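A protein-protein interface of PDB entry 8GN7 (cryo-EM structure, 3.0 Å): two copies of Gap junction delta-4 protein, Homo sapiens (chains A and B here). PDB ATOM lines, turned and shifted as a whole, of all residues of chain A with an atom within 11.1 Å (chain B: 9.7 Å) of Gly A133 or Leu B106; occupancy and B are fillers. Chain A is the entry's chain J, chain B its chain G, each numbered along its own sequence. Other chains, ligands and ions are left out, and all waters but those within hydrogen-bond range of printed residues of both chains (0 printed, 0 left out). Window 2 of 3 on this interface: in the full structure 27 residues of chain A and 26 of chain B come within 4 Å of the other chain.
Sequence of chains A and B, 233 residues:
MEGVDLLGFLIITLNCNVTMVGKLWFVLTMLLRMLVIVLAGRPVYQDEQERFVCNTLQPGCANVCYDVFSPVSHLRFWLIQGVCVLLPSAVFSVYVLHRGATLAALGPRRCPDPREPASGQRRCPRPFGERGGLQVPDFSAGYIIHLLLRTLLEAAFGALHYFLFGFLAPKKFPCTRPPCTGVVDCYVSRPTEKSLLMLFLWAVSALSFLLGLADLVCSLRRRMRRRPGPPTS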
ATOM      1  N   VAL A   4      -0.306 -19.664 -12.390  1.00  0.00           N
ATOM      2  CA  VAL A   4      -0.302 -18.666 -11.333  1.00  0.00           C
ATOM      3  C   VAL A   4       1.123 -18.527 -10.802  1.00  0.00           C
ATOM      4  O   VAL A   4       1.948 -19.431 -10.939  1.00  0.00           O
ATOM      5  CB  VAL A   4      -1.291 -19.013 -10.200  1.00  0.00           C
ATOM      6  CG1 VAL A   4      -0.684 -20.031  -9.246  1.00  0.00           C
ATOM      7  CG2 VAL A   4      -1.721 -17.757  -9.454  1.00  0.00           C
ATOM      8  N   PHE A   9       1.116 -16.694  -3.710  1.00  0.00           N
ATOM      9  CA  PHE A   9       0.784 -17.902  -2.966  1.00  0.00           C
ATOM     10  C   PHE A   9       1.531 -17.989  -1.643  1.00  0.00           C
ATOM     11  O   PHE A   9       1.030 -18.610  -0.700  1.00  0.00           O
ATOM     12  CB  PHE A   9       1.087 -19.137  -3.816  1.00  0.00           C
ATOM     13  CG  PHE A   9       0.700 -20.430  -3.164  1.00  0.00           C
ATOM     14  CD1 PHE A   9       1.669 -21.291  -2.677  1.00  0.00           C
ATOM     15  CD2 PHE A   9      -0.629 -20.789  -3.041  1.00  0.00           C
ATOM     16  CE1 PHE A   9       1.319 -22.484  -2.079  1.00  0.00           C
ATOM     17  CE2 PHE A   9      -0.985 -21.982  -2.443  1.00  0.00           C
ATOM     18  CZ  PHE A   9      -0.009 -22.831  -1.962  1.00  0.00           C
ATOM     19  N   ILE A  12      -0.631 -15.437   0.742  1.00  0.00           N
ATOM     20  CA  ILE A  12      -1.976 -15.892   1.078  1.00  0.00           C
ATOM     21  C   ILE A  12      -1.914 -17.078   2.032  1.00  0.00           C
ATOM     22  O   ILE A  12      -2.750 -17.208   2.935  1.00  0.00           O
ATOM     23  CB  ILE A  12      -2.761 -16.212  -0.208  1.00  0.00           C
ATOM     24  CG1 ILE A  12      -3.639 -15.023  -0.601  1.00  0.00           C
ATOM     25  CG2 ILE A  12      -3.617 -17.448  -0.038  1.00  0.00           C
ATOM     26  CD1 ILE A  12      -2.896 -13.716  -0.701  1.00  0.00           C
ATOM     27  N   THR A  13      -0.921 -17.952   1.861  1.00  0.00           N
ATOM     28  CA  THR A  13      -0.711 -19.028   2.824  1.00  0.00           C
ATOM     29  C   THR A  13      -0.405 -18.469   4.208  1.00  0.00           C
ATOM     30  O   THR A  13      -0.922 -18.966   5.216  1.00  0.00           O
ATOM     31  CB  THR A  13       0.423 -19.938   2.354  1.00  0.00           C
ATOM     32  OG1 THR A  13       0.092 -20.490   1.076  1.00  0.00           O
ATOM     33  CG2 THR A  13       0.647 -21.070   3.343  1.00  0.00           C
ATOM     34  N   ASN A  15      -1.098 -15.279   5.242  1.00  0.00           N
ATOM     35  CA  ASN A  15      -2.200 -14.427   5.681  1.00  0.00           C
ATOM     36  C   ASN A  15      -3.484 -15.246   5.535  1.00  0.00           C
ATOM     37  O   ASN A  15      -4.412 -14.928   4.799  1.00  0.00           O
ATOM     38  CB  ASN A  15      -2.175 -13.110   4.883  1.00  0.00           C
ATOM     39  CG  ASN A  15      -3.492 -12.282   4.881  1.00  0.00           C
ATOM     40  OD1 ASN A  15      -4.581 -12.698   5.266  1.00  0.00           O
ATOM     41  ND2 ASN A  15      -3.339 -11.037   4.442  1.00  0.00           N
ATOM     42  N   CYS A  16      -3.438 -16.455   6.076  1.00  0.00           N
ATOM     43  CA  CYS A  16      -4.625 -17.269   6.286  1.00  0.00           C
ATOM     44  C   CYS A  16      -4.505 -18.117   7.542  1.00  0.00           C
ATOM     45  O   CYS A  16      -5.483 -18.766   7.928  1.00  0.00           O
ATOM     46  CB  CYS A  16      -4.892 -18.177   5.075  1.00  0.00           C
ATOM     47  SG  CYS A  16      -5.896 -17.425   3.768  1.00  0.00           S
ATOM     48  N   PRO A 108       0.238 -30.427  -7.717  1.00  0.00           N
ATOM     49  CA  PRO A 108      -0.949 -31.240  -7.430  1.00  0.00           C
ATOM     50  C   PRO A 108      -0.749 -32.714  -7.770  1.00  0.00           C
ATOM     51  O   PRO A 108      -1.734 -33.451  -7.827  1.00  0.00           O
ATOM     52  CB  PRO A 108      -2.027 -30.618  -8.324  1.00  0.00           C
ATOM     53  CG  PRO A 108      -1.274 -29.922  -9.406  1.00  0.00           C
ATOM     54  CD  PRO A 108      -0.018 -29.425  -8.765  1.00  0.00           C
ATOM     55  N   GLY A 133     -10.545 -20.282  -5.598  1.00  0.00           N
ATOM     56  CA  GLY A 133     -10.472 -21.721  -5.428  1.00  0.00           C
ATOM     57  C   GLY A 133      -9.051 -22.241  -5.348  1.00  0.00           C
ATOM     58  O   GLY A 133      -8.602 -22.986  -6.218  1.00  0.00           O
ATOM     59  N   LEU A 134      -8.340 -21.843  -4.298  1.00  0.00           N
ATOM     60  CA  LEU A 134      -6.959 -22.252  -4.099  1.00  0.00           C
ATOM     61  C   LEU A 134      -6.913 -23.524  -3.252  1.00  0.00           C
ATOM     62  O   LEU A 134      -7.945 -24.114  -2.919  1.00  0.00           O
ATOM     63  CB  LEU A 134      -6.159 -21.113  -3.470  1.00  0.00           C
ATOM     64  CG  LEU A 134      -5.648 -20.032  -4.425  1.00  0.00           C
ATOM     65  CD1 LEU A 134      -4.504 -19.253  -3.793  1.00  0.00           C
ATOM     66  CD2 LEU A 134      -5.219 -20.638  -5.754  1.00  0.00           C
ATOM     67  N   GLN A 135      -5.708 -23.959  -2.896  1.00  0.00           N
ATOM     68  CA  GLN A 135      -5.482 -25.172  -2.114  1.00  0.00           C
ATOM     69  C   GLN A 135      -4.507 -24.890  -0.978  1.00  0.00           C
ATOM     70  O   GLN A 135      -3.526 -25.606  -0.766  1.00  0.00           O
ATOM     71  CB  GLN A 135      -4.975 -26.306  -3.001  1.00  0.00           C
ATOM     72  CG  GLN A 135      -5.349 -27.691  -2.502  1.00  0.00           C
ATOM     73  CD  GLN A 135      -6.816 -27.800  -2.137  1.00  0.00           C
ATOM     74  OE1 GLN A 135      -7.692 -27.457  -2.931  1.00  0.00           O
ATOM     75  NE2 GLN A 135      -7.092 -28.280  -0.930  1.00  0.00           N
ATOM     76  N   VAL A 136      -4.774 -23.818  -0.239  1.00  0.00           N
ATOM     77  CA  VAL A 136      -3.860 -23.361   0.816  1.00  0.00           C
ATOM     78  C   VAL A 136      -3.792 -24.407   1.922  1.00  0.00           C
ATOM     79  O   VAL A 136      -4.843 -24.905   2.371  1.00  0.00           O
ATOM     80  CB  VAL A 136      -4.324 -22.005   1.372  1.00  0.00           C
ATOM     81  CG1 VAL A 136      -3.611 -21.681   2.675  1.00  0.00           C
ATOM     82  CG2 VAL A 136      -4.104 -20.919   0.344  1.00  0.00           C
ATOM     83  N   PRO A 137      -2.604 -24.782   2.392  1.00  0.00           N
ATOM     84  CA  PRO A 137      -2.513 -25.731   3.505  1.00  0.00           C
ATOM     85  C   PRO A 137      -3.009 -25.126   4.809  1.00  0.00           C
ATOM     86  O   PRO A 137      -3.090 -23.907   4.979  1.00  0.00           O
ATOM     87  CB  PRO A 137      -1.017 -26.058   3.574  1.00  0.00           C
ATOM     88  CG  PRO A 137      -0.342 -24.885   2.936  1.00  0.00           C
ATOM     89  CD  PRO A 137      -1.281 -24.378   1.885  1.00  0.00           C
ATOM     90  N   LEU B   6      -0.885 -11.333  -7.974  1.00  0.00           N
ATOM     91  CA  LEU B   6      -1.556 -10.988  -6.725  1.00  0.00           C
ATOM     92  C   LEU B   6      -0.768  -9.949  -5.933  1.00  0.00           C
ATOM     93  O   LEU B   6      -1.351  -9.221  -5.124  1.00  0.00           O
ATOM     94  CB  LEU B   6      -1.819 -12.268  -5.910  1.00  0.00           C
ATOM     95  CG  LEU B   6      -2.492 -12.362  -4.535  1.00  0.00           C
ATOM     96  CD1 LEU B   6      -2.665 -13.826  -4.222  1.00  0.00           C
ATOM     97  CD2 LEU B   6      -1.700 -11.717  -3.405  1.00  0.00           C
ATOM     98  N   HIS B  98      -5.173  -7.541   5.623  1.00  0.00           N
ATOM     99  CA  HIS B  98      -5.831  -8.757   6.085  1.00  0.00           C
ATOM    100  C   HIS B  98      -7.106  -9.040   5.304  1.00  0.00           C
ATOM    101  O   HIS B  98      -7.365 -10.192   4.943  1.00  0.00           O
ATOM    102  CB  HIS B  98      -6.140  -8.656   7.579  1.00  0.00           C
ATOM    103  CG  HIS B  98      -7.119  -9.678   8.065  1.00  0.00           C
ATOM    104  ND1 HIS B  98      -6.746 -10.951   8.438  1.00  0.00           N
ATOM    105  CD2 HIS B  98      -8.461  -9.614   8.242  1.00  0.00           C
ATOM    106  CE1 HIS B  98      -7.813 -11.627   8.822  1.00  0.00           C
ATOM    107  NE2 HIS B  98      -8.867 -10.839   8.711  1.00  0.00           N
ATOM    108  N   ARG B  99      -7.912  -8.012   5.039  1.00  0.00           N
ATOM    109  CA  ARG B  99      -9.175  -8.208   4.341  1.00  0.00           C
ATOM    110  C   ARG B  99      -9.008  -8.402   2.839  1.00  0.00           C
ATOM    111  O   ARG B  99      -9.737  -9.203   2.245  1.00  0.00           O
ATOM    112  CB  ARG B  99     -10.106  -7.021   4.601  1.00  0.00           C
ATOM    113  CG  ARG B  99     -11.533  -7.241   4.140  1.00  0.00           C
ATOM    114  CD  ARG B  99     -12.378  -7.862   5.238  1.00  0.00           C
ATOM    115  NE  ARG B  99     -13.634  -7.147   5.423  1.00  0.00           N
ATOM    116  CZ  ARG B  99     -14.704  -7.303   4.656  1.00  0.00           C
ATOM    117  NH1 ARG B  99     -14.708  -8.147   3.637  1.00  0.00           N
ATOM    118  NH2 ARG B  99     -15.799  -6.594   4.918  1.00  0.00           N
ATOM    119  N   GLY B 100      -8.070  -7.689   2.210  1.00  0.00           N
ATOM    120  CA  GLY B 100      -7.915  -7.786   0.769  1.00  0.00           C
ATOM    121  C   GLY B 100      -7.335  -9.097   0.286  1.00  0.00           C
ATOM    122  O   GLY B 100      -7.768  -9.624  -0.741  1.00  0.00           O
ATOM    123  N   ALA B 101      -6.354  -9.640   1.005  1.00  0.00           N
ATOM    124  CA  ALA B 101      -5.729 -10.898   0.619  1.00  0.00           C
ATOM    125  C   ALA B 101      -6.569 -12.114   0.977  1.00  0.00           C
ATOM    126  O   ALA B 101      -6.342 -13.193   0.418  1.00  0.00           O
ATOM    127  CB  ALA B 101      -4.348 -11.023   1.268  1.00  0.00           C
ATOM    128  N   THR B 102      -7.532 -11.968   1.885  1.00  0.00           N
ATOM    129  CA  THR B 102      -8.459 -13.033   2.236  1.00  0.00           C
ATOM    130  C   THR B 102      -9.696 -13.024   1.348  1.00  0.00           C
ATOM    131  O   THR B 102     -10.553 -13.905   1.476  1.00  0.00           O
ATOM    132  CB  THR B 102      -8.861 -12.910   3.710  1.00  0.00           C
ATOM    133  OG1 THR B 102      -7.742 -12.440   4.470  1.00  0.00           O
ATOM    134  CG2 THR B 102      -9.295 -14.259   4.268  1.00  0.00           C
ATOM    135  N   LEU B 103      -9.800 -12.052   0.439  1.00  0.00           N
ATOM    136  CA  LEU B 103     -10.923 -11.950  -0.477  1.00  0.00           C
ATOM    137  C   LEU B 103     -10.633 -12.526  -1.854  1.00  0.00           C
ATOM    138  O   LEU B 103     -11.560 -13.014  -2.507  1.00  0.00           O
ATOM    139  CB  LEU B 103     -11.350 -10.480  -0.625  1.00  0.00           C
ATOM    140  CG  LEU B 103     -12.594 -10.135  -1.447  1.00  0.00           C
ATOM    141  CD1 LEU B 103     -13.377  -9.022  -0.768  1.00  0.00           C
ATOM    142  CD2 LEU B 103     -12.218  -9.726  -2.864  1.00  0.00           C
ATOM    143  N   ALA B 104      -9.381 -12.485  -2.306  1.00  0.00           N
ATOM    144  CA  ALA B 104      -9.017 -13.055  -3.595  1.00  0.00           C
ATOM    145  C   ALA B 104      -8.795 -14.559  -3.541  1.00  0.00           C
ATOM    146  O   ALA B 104      -8.756 -15.202  -4.595  1.00  0.00           O
ATOM    147  CB  ALA B 104      -7.753 -12.377  -4.135  1.00  0.00           C
ATOM    148  N   ALA B 105      -8.644 -15.130  -2.343  1.00  0.00           N
ATOM    149  CA  ALA B 105      -8.465 -16.574  -2.232  1.00  0.00           C
ATOM    150  C   ALA B 105      -9.707 -17.322  -2.695  1.00  0.00           C
ATOM    151  O   ALA B 105      -9.607 -18.329  -3.408  1.00  0.00           O
ATOM    152  CB  ALA B 105      -8.115 -16.949  -0.793  1.00  0.00           C
ATOM    153  N   LEU B 106     -10.891 -16.847  -2.299  1.00  0.00           N
ATOM    154  CA  LEU B 106     -12.126 -17.504  -2.715  1.00  0.00           C
ATOM    155  C   LEU B 106     -12.413 -17.262  -4.192  1.00  0.00           C
ATOM    156  O   LEU B 106     -12.982 -18.125  -4.869  1.00  0.00           O
ATOM    157  CB  LEU B 106     -13.292 -17.024  -1.852  1.00  0.00           C
ATOM    158  CG  LEU B 106     -13.197 -17.344  -0.358  1.00  0.00           C
ATOM    159  CD1 LEU B 106     -12.711 -16.136   0.426  1.00  0.00           C
ATOM    160  CD2 LEU B 106     -14.534 -17.834   0.177  1.00  0.00           C
ATOM    161  N   GLY B 107     -12.030 -16.096  -4.707  1.00  0.00           N
ATOM    162  CA  GLY B 107     -12.247 -15.770  -6.096  1.00  0.00           C
ATOM    163  C   GLY B 107     -13.642 -15.242  -6.355  1.00  0.00           C
ATOM    164  O   GLY B 107     -14.457 -15.096  -5.438  1.00  0.00           O
ATOM    165  N   PRO B 108     -13.947 -14.939  -7.625  1.00  0.00           N
ATOM    166  CA  PRO B 108     -15.254 -14.408  -8.033  1.00  0.00           C
ATOM    167  C   PRO B 108     -16.390 -15.403  -7.809  1.00  0.00           C
ATOM    168  O   PRO B 108     -17.477 -15.196  -8.347  1.00  0.00           O
ATOM    169  CB  PRO B 108     -15.070 -14.124  -9.528  1.00  0.00           C
ATOM    170  CG  PRO B 108     -13.939 -15.000  -9.948  1.00  0.00           C
ATOM    171  CD  PRO B 108     -13.025 -15.072  -8.767  1.00  0.00           C
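Of the 12 printed residues of chain B, 6 touch a printed residue of chain A.
Printed residues of chain B that touch a printed residue of chain A: Leu B6, His B98, Ala B101, Thr B102, Ala B105 and Leu B106.
Hydrophobic or aromatic side chains of chain B within 4 Å of the printed part of chain A: Leu B6 and Ala B101.
Hydrophobic or aromatic side chains of chain A within 4 Å of the printed part of chain B: Ile A12.
Along chain A the printed residues that touch a printed residue of chain B span positions 12 to 134.
Among the printed residues, 8 pairs touch across the chains.
The side-chain sulfur of Cys A16 lies close to the backbone carbonyl oxygen of Ile A12 (3.3 Å).
Leu B106 touches one residue of chain A.
No residue of chain A comes within 4 Å of Ala B104.
Ala B105 touches just these residues of chain A: Gly A133 and Leu A134.
No residue of chain A comes within 4 Å of Pro B108.
Printed residues of chain A within 4 Å of Leu B6: Ile A12 (3.5 Å).
Of the printed residues of chain A, His B98 touches Asn A15 (3.8 Å).
Thr A13 touches none of the printed residues of chain B.
Pro A137 touches none of the printed residues of chain B.
The nearest printed residue of chain A that does not touch His B98 is Cys A16 (6.8 Å).
Ile A12 touches Leu B6 (CD1 to CD1, 3.5 Å).
CG1 of Ile A12 touches O of Ala B101, 3.4 Å away.
His B98 touches Asn A15 (CA to ND2, 3.8 Å).
Asn A15 touches Ala B101.
Ala B105 touches Leu A134 (O to N, 3.8 Å).
OG1 of Thr B102 lies within hydrogen-bond range of OD1 of Asn A15 (3.3 Å).
O of Ala B105 sits at hydrogen-bond distance from N of Gly A133 (3.1 Å).
The backbone NH of Gly A133 lies within hydrogen-bond range of the backbone carbonyl oxygen of Leu B106, at 3.3 Å.
1 position is printed for both chains.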
